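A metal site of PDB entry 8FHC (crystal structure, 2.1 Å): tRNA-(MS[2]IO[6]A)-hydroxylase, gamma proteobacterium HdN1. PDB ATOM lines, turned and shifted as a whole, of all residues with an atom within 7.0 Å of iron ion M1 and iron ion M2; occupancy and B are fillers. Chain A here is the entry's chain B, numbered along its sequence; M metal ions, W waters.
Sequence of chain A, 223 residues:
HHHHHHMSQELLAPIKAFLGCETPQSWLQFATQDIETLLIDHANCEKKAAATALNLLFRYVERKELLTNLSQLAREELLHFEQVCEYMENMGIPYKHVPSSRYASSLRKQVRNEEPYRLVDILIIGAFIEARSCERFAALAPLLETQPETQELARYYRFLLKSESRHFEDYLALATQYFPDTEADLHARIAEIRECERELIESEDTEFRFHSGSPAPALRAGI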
ATOM      1  N   HIS A  42     -35.899   3.278  20.140  1.00  0.00           N
ATOM      2  CA  HIS A  42     -34.529   3.457  20.610  1.00  0.00           C
ATOM      3  C   HIS A  42     -34.516   4.035  22.029  1.00  0.00           C
ATOM      4  O   HIS A  42     -33.857   3.490  22.914  1.00  0.00           O
ATOM      5  CB  HIS A  42     -33.771   4.332  19.606  1.00  0.00           C
ATOM      6  CG  HIS A  42     -32.348   4.612  19.951  1.00  0.00           C
ATOM      7  ND1 HIS A  42     -31.589   5.413  19.125  1.00  0.00           N
ATOM      8  CD2 HIS A  42     -31.530   4.259  20.965  1.00  0.00           C
ATOM      9  CE1 HIS A  42     -30.356   5.520  19.627  1.00  0.00           C
ATOM     10  NE2 HIS A  42     -30.309   4.841  20.745  1.00  0.00           N
ATOM     11  N   CYS A  45     -35.539   1.605  24.389  1.00  0.00           N
ATOM     12  CA  CYS A  45     -34.537   0.541  24.560  1.00  0.00           C
ATOM     13  C   CYS A  45     -33.441   0.966  25.535  1.00  0.00           C
ATOM     14  O   CYS A  45     -32.938   0.130  26.272  1.00  0.00           O
ATOM     15  CB  CYS A  45     -33.884   0.145  23.255  1.00  0.00           C
ATOM     16  SG  CYS A  45     -34.985  -0.833  22.213  1.00  0.00           S
ATOM     17  N   GLU A  46     -33.066   2.237  25.512  1.00  0.00           N
ATOM     18  CA  GLU A  46     -32.080   2.772  26.444  1.00  0.00           C
ATOM     19  C   GLU A  46     -32.597   2.596  27.876  1.00  0.00           C
ATOM     20  O   GLU A  46     -31.845   2.154  28.750  1.00  0.00           O
ATOM     21  CB  GLU A  46     -31.783   4.219  26.077  1.00  0.00           C
ATOM     22  CG  GLU A  46     -31.200   4.379  24.665  1.00  0.00           C
ATOM     23  CD  GLU A  46     -29.816   3.806  24.377  1.00  0.00           C
ATOM     24  OE1 GLU A  46     -29.227   3.204  25.282  1.00  0.00           O
ATOM     25  OE2 GLU A  46     -29.284   4.013  23.252  1.00  0.00           O
ATOM     26  N   ALA A  49     -32.308  -1.021  28.925  1.00  0.00           N
ATOM     27  CA  ALA A  49     -30.937  -1.350  29.239  1.00  0.00           C
ATOM     28  C   ALA A  49     -30.630  -0.912  30.679  1.00  0.00           C
ATOM     29  O   ALA A  49     -30.003  -1.656  31.437  1.00  0.00           O
ATOM     30  CB  ALA A  49     -30.040  -0.695  28.226  1.00  0.00           C
ATOM     31  N   LEU A  73     -22.694   1.423  33.761  1.00  0.00           N
ATOM     32  CA  LEU A  73     -23.390   1.159  32.518  1.00  0.00           C
ATOM     33  C   LEU A  73     -24.826   1.724  32.573  1.00  0.00           C
ATOM     34  O   LEU A  73     -25.253   2.379  31.640  1.00  0.00           O
ATOM     35  CB  LEU A  73     -23.334  -0.352  32.294  1.00  0.00           C
ATOM     36  CG  LEU A  73     -23.855  -0.901  30.975  1.00  0.00           C
ATOM     37  CD1 LEU A  73     -23.165  -2.215  30.636  1.00  0.00           C
ATOM     38  CD2 LEU A  73     -25.371  -1.113  30.999  1.00  0.00           C
ATOM     39  N   GLU A  76     -24.819   5.243  31.966  1.00  0.00           N
ATOM     40  CA  GLU A  76     -24.554   5.604  30.571  1.00  0.00           C
ATOM     41  C   GLU A  76     -25.797   5.424  29.712  1.00  0.00           C
ATOM     42  O   GLU A  76     -26.031   6.172  28.764  1.00  0.00           O
ATOM     43  CB  GLU A  76     -23.384   4.800  30.002  1.00  0.00           C
ATOM     44  CG  GLU A  76     -22.039   5.268  30.507  1.00  0.00           C
ATOM     45  CD  GLU A  76     -20.908   4.283  30.262  1.00  0.00           C
ATOM     46  OE1 GLU A  76     -20.041   4.131  31.145  1.00  0.00           O
ATOM     47  OE2 GLU A  76     -20.887   3.674  29.168  1.00  0.00           O
ATOM     48  N   GLU A  77     -26.611   4.407  30.015  1.00  0.00           N
ATOM     49  CA  GLU A  77     -27.832   4.178  29.266  1.00  0.00           C
ATOM     50  C   GLU A  77     -28.818   5.322  29.456  1.00  0.00           C
ATOM     51  O   GLU A  77     -29.501   5.708  28.503  1.00  0.00           O
ATOM     52  CB  GLU A  77     -28.479   2.850  29.669  1.00  0.00           C
ATOM     53  CG  GLU A  77     -27.583   1.632  29.556  1.00  0.00           C
ATOM     54  CD  GLU A  77     -27.178   1.326  28.123  1.00  0.00           C
ATOM     55  OE1 GLU A  77     -27.557   2.085  27.232  1.00  0.00           O
ATOM     56  OE2 GLU A  77     -26.514   0.319  27.929  1.00  0.00           O
ATOM     57  N   LEU A  78     -28.904   5.836  30.703  1.00  0.00           N
ATOM     58  CA  LEU A  78     -29.776   6.953  31.043  1.00  0.00           C
ATOM     59  C   LEU A  78     -29.373   8.212  30.293  1.00  0.00           C
ATOM     60  O   LEU A  78     -30.223   8.984  29.822  1.00  0.00           O
ATOM     61  CB  LEU A  78     -29.754   7.168  32.558  1.00  0.00           C
ATOM     62  CG  LEU A  78     -30.540   6.123  33.355  1.00  0.00           C
ATOM     63  CD1 LEU A  78     -30.205   6.179  34.828  1.00  0.00           C
ATOM     64  CD2 LEU A  78     -32.022   6.296  33.145  1.00  0.00           C
ATOM     65  N   HIS A  80     -27.948   8.055  27.494  1.00  0.00           N
ATOM     66  CA  HIS A  80     -28.372   7.745  26.131  1.00  0.00           C
ATOM     67  C   HIS A  80     -29.843   8.083  25.945  1.00  0.00           C
ATOM     68  O   HIS A  80     -30.205   8.732  24.970  1.00  0.00           O
ATOM     69  CB  HIS A  80     -28.032   6.287  25.803  1.00  0.00           C
ATOM     70  CG  HIS A  80     -26.572   6.041  25.599  1.00  0.00           C
ATOM     71  ND1 HIS A  80     -26.081   4.751  25.479  1.00  0.00           N
ATOM     72  CD2 HIS A  80     -25.518   6.873  25.483  1.00  0.00           C
ATOM     73  CE1 HIS A  80     -24.770   4.809  25.285  1.00  0.00           C
ATOM     74  NE2 HIS A  80     -24.396   6.093  25.287  1.00  0.00           N
ATOM     75  N   PHE A  81     -30.687   7.697  26.909  1.00  0.00           N
ATOM     76  CA  PHE A  81     -32.087   8.033  26.882  1.00  0.00           C
ATOM     77  C   PHE A  81     -32.295   9.543  26.720  1.00  0.00           C
ATOM     78  O   PHE A  81     -33.045   9.971  25.845  1.00  0.00           O
ATOM     79  CB  PHE A  81     -32.796   7.478  28.133  1.00  0.00           C
ATOM     80  CG  PHE A  81     -34.197   7.986  28.341  1.00  0.00           C
ATOM     81  CD1 PHE A  81     -35.229   7.565  27.522  1.00  0.00           C
ATOM     82  CD2 PHE A  81     -34.486   8.882  29.360  1.00  0.00           C
ATOM     83  CE1 PHE A  81     -36.520   8.028  27.729  1.00  0.00           C
ATOM     84  CE2 PHE A  81     -35.775   9.374  29.535  1.00  0.00           C
ATOM     85  CZ  PHE A  81     -36.794   8.940  28.724  1.00  0.00           C
ATOM     86  N   GLU A 130     -26.540  -5.900  23.516  1.00  0.00           N
ATOM     87  CA  GLU A 130     -25.587  -4.819  23.266  1.00  0.00           C
ATOM     88  C   GLU A 130     -24.846  -5.056  21.951  1.00  0.00           C
ATOM     89  O   GLU A 130     -24.578  -4.103  21.225  1.00  0.00           O
ATOM     90  CB  GLU A 130     -24.588  -4.678  24.415  1.00  0.00           C
ATOM     91  CG  GLU A 130     -25.233  -4.311  25.761  1.00  0.00           C
ATOM     92  CD  GLU A 130     -25.983  -2.989  25.753  1.00  0.00           C
ATOM     93  OE1 GLU A 130     -25.452  -2.018  26.250  1.00  0.00           O
ATOM     94  OE2 GLU A 130     -27.137  -2.961  25.294  1.00  0.00           O
ATOM     95  N   SER A 133     -27.335  -4.277  19.116  1.00  0.00           N
ATOM     96  CA  SER A 133     -27.488  -2.847  18.985  1.00  0.00           C
ATOM     97  C   SER A 133     -26.282  -2.250  18.255  1.00  0.00           C
ATOM     98  O   SER A 133     -26.420  -1.478  17.315  1.00  0.00           O
ATOM     99  CB  SER A 133     -27.724  -2.230  20.345  1.00  0.00           C
ATOM    100  OG  SER A 133     -28.872  -2.827  20.981  1.00  0.00           O
ATOM    101  N   PHE A 137     -26.661  -0.215  14.686  1.00  0.00           N
ATOM    102  CA  PHE A 137     -26.269   1.175  14.502  1.00  0.00           C
ATOM    103  C   PHE A 137     -25.203   1.323  13.413  1.00  0.00           C
ATOM    104  O   PHE A 137     -25.238   2.288  12.647  1.00  0.00           O
ATOM    105  CB  PHE A 137     -25.690   1.773  15.780  1.00  0.00           C
ATOM    106  CG  PHE A 137     -26.619   1.972  16.960  1.00  0.00           C
ATOM    107  CD1 PHE A 137     -27.807   2.651  16.844  1.00  0.00           C
ATOM    108  CD2 PHE A 137     -26.218   1.570  18.229  1.00  0.00           C
ATOM    109  CE1 PHE A 137     -28.633   2.862  17.951  1.00  0.00           C
ATOM    110  CE2 PHE A 137     -27.029   1.797  19.335  1.00  0.00           C
ATOM    111  CZ  PHE A 137     -28.235   2.439  19.190  1.00  0.00           C
ATOM    112  N   TYR A 156     -24.369  10.413  15.381  1.00  0.00           N
ATOM    113  CA  TYR A 156     -24.740   9.893  16.688  1.00  0.00           C
ATOM    114  C   TYR A 156     -24.613   8.378  16.695  1.00  0.00           C
ATOM    115  O   TYR A 156     -24.040   7.816  17.617  1.00  0.00           O
ATOM    116  CB  TYR A 156     -26.145  10.348  17.095  1.00  0.00           C
ATOM    117  CG  TYR A 156     -26.570   9.906  18.469  1.00  0.00           C
ATOM    118  CD1 TYR A 156     -25.712  10.005  19.553  1.00  0.00           C
ATOM    119  CD2 TYR A 156     -27.844   9.389  18.707  1.00  0.00           C
ATOM    120  CE1 TYR A 156     -26.097   9.619  20.826  1.00  0.00           C
ATOM    121  CE2 TYR A 156     -28.231   8.975  19.987  1.00  0.00           C
ATOM    122  CZ  TYR A 156     -27.356   9.075  21.047  1.00  0.00           C
ATOM    123  OH  TYR A 156     -27.722   8.678  22.319  1.00  0.00           O
ATOM    124  N   LEU A 160     -22.302   5.931  19.079  1.00  0.00           N
ATOM    125  CA  LEU A 160     -22.821   4.941  20.006  1.00  0.00           C
ATOM    126  C   LEU A 160     -22.077   3.621  19.875  1.00  0.00           C
ATOM    127  O   LEU A 160     -22.110   2.810  20.804  1.00  0.00           O
ATOM    128  CB  LEU A 160     -24.322   4.743  19.773  1.00  0.00           C
ATOM    129  CG  LEU A 160     -25.247   5.821  20.342  1.00  0.00           C
ATOM    130  CD1 LEU A 160     -26.658   5.588  19.850  1.00  0.00           C
ATOM    131  CD2 LEU A 160     -25.210   5.845  21.873  1.00  0.00           C
ATOM    132  N   SER A 163     -19.715   3.124  22.880  1.00  0.00           N
ATOM    133  CA  SER A 163     -20.433   2.697  24.076  1.00  0.00           C
ATOM    134  C   SER A 163     -20.827   1.220  24.017  1.00  0.00           C
ATOM    135  O   SER A 163     -20.485   0.428  24.891  1.00  0.00           O
ATOM    136  CB  SER A 163     -21.671   3.537  24.208  1.00  0.00           C
ATOM    137  OG  SER A 163     -21.886   3.851  25.567  1.00  0.00           O
ATOM    138  N   GLU A 164     -21.552   0.851  22.952  1.00  0.00           N
ATOM    139  CA  GLU A 164     -22.223  -0.428  22.866  1.00  0.00           C
ATOM    140  C   GLU A 164     -21.188  -1.541  22.824  1.00  0.00           C
ATOM    141  O   GLU A 164     -21.389  -2.577  23.454  1.00  0.00           O
ATOM    142  CB  GLU A 164     -23.190  -0.487  21.674  1.00  0.00           C
ATOM    143  CG  GLU A 164     -24.449   0.329  21.875  1.00  0.00           C
ATOM    144  CD  GLU A 164     -25.042   0.210  23.273  1.00  0.00           C
ATOM    145  OE1 GLU A 164     -25.278  -0.940  23.697  1.00  0.00           O
ATOM    146  OE2 GLU A 164     -25.210   1.267  23.975  1.00  0.00           O
ATOM    147  N   SER A 165     -20.089  -1.303  22.108  1.00  0.00           N
ATOM    148  CA  SER A 165     -19.021  -2.283  22.002  1.00  0.00           C
ATOM    149  C   SER A 165     -18.405  -2.578  23.370  1.00  0.00           C
ATOM    150  O   SER A 165     -18.091  -3.724  23.653  1.00  0.00           O
ATOM    151  CB  SER A 165     -17.994  -1.876  20.947  1.00  0.00           C
ATOM    152  OG  SER A 165     -17.210  -0.770  21.377  1.00  0.00           O
ATOM    153  N   HIS A 167     -20.079  -2.151  26.265  1.00  0.00           N
ATOM    154  CA  HIS A 167     -21.169  -2.737  27.027  1.00  0.00           C
ATOM    155  C   HIS A 167     -21.248  -4.241  26.758  1.00  0.00           C
ATOM    156  O   HIS A 167     -21.446  -5.034  27.684  1.00  0.00           O
ATOM    157  CB  HIS A 167     -22.474  -1.995  26.725  1.00  0.00           C
ATOM    158  CG  HIS A 167     -22.507  -0.586  27.250  1.00  0.00           C
ATOM    159  ND1 HIS A 167     -23.598   0.225  27.116  1.00  0.00           N
ATOM    160  CD2 HIS A 167     -21.623   0.134  27.970  1.00  0.00           C
ATOM    161  CE1 HIS A 167     -23.367   1.405  27.692  1.00  0.00           C
ATOM    162  NE2 HIS A 167     -22.182   1.357  28.245  1.00  0.00           N
ATOM    163  N   PHE A 168     -21.119  -4.622  25.481  1.00  0.00           N
ATOM    164  CA  PHE A 168     -21.024  -6.019  25.074  1.00  0.00           C
ATOM    165  C   PHE A 168     -19.897  -6.711  25.831  1.00  0.00           C
ATOM    166  O   PHE A 168     -20.078  -7.780  26.424  1.00  0.00           O
ATOM    167  CB  PHE A 168     -20.804  -6.109  23.569  1.00  0.00           C
ATOM    168  CG  PHE A 168     -20.158  -7.390  23.104  1.00  0.00           C
ATOM    169  CD1 PHE A 168     -20.770  -8.617  23.284  1.00  0.00           C
ATOM    170  CD2 PHE A 168     -18.880  -7.364  22.555  1.00  0.00           C
ATOM    171  CE1 PHE A 168     -20.148  -9.788  22.887  1.00  0.00           C
ATOM    172  CE2 PHE A 168     -18.251  -8.541  22.162  1.00  0.00           C
ATOM    173  CZ  PHE A 168     -18.882  -9.750  22.330  1.00  0.00           C
ATOM    174  N   TYR A 171     -20.637  -7.121  29.714  1.00  0.00           N
ATOM    175  CA  TYR A 171     -21.564  -8.220  29.968  1.00  0.00           C
ATOM    176  C   TYR A 171     -20.903  -9.582  29.751  1.00  0.00           C
ATOM    177  O   TYR A 171     -21.060 -10.482  30.560  1.00  0.00           O
ATOM    178  CB  TYR A 171     -22.856  -8.049  29.132  1.00  0.00           C
ATOM    179  CG  TYR A 171     -23.936  -7.217  29.778  1.00  0.00           C
ATOM    180  CD1 TYR A 171     -24.554  -7.653  30.945  1.00  0.00           C
ATOM    181  CD2 TYR A 171     -24.329  -5.996  29.240  1.00  0.00           C
ATOM    182  CE1 TYR A 171     -25.521  -6.887  31.577  1.00  0.00           C
ATOM    183  CE2 TYR A 171     -25.310  -5.209  29.852  1.00  0.00           C
ATOM    184  CZ  TYR A 171     -25.896  -5.671  31.026  1.00  0.00           C
ATOM    185  OH  TYR A 171     -26.869  -4.969  31.685  1.00  0.00           O
HETATM  186 FE    FE M   1     -27.158   2.749  25.250  1.00  0.00          FE
HETATM  187 FE    FE M   2     -25.598  -0.108  26.009  1.00  0.00          FE
HETATM  188  O   HOH W   1     -28.085  -0.009  24.872  1.00  0.00           O
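The side-chain carboxylate (OE2) of Glu 46 lies within hydrogen-bond range of a ring nitrogen (NE2) of His 42 (2.8 Å). NE2 of His 80 sits close to OG of Ser 163, 3.4 Å away. A ring nitrogen (NE2) of His 167 is in hydrogen-bond range of the side-chain carboxylate (OE2) of Glu 76.
Of the 21 residues printed, 4 come within 4 Å of iron ion M1. Along chain A the residues within 4 Å of iron ion M1 span positions 46 to 164.
Of the 21 residues printed, 4 come within 4 Å of iron ion M2. The nearest printed residue that does not touch iron ion M2 is His 80 (4.9 Å).
Iron ion M1 is bound by OE1 of Glu 46, OE1 of Glu 77 and ND1 of His 80. Slightly farther from iron ion M1 lies OE2 of Glu 164 (2.8 Å).
Iron ion M2 is bound by OE1 of Glu 130, OE2 of Glu 77, ND1 of His 167, OE1 of Glu 164 and OE2 of Glu 164. Slightly farther from iron ion M2 lies water W1 (2.7 Å).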
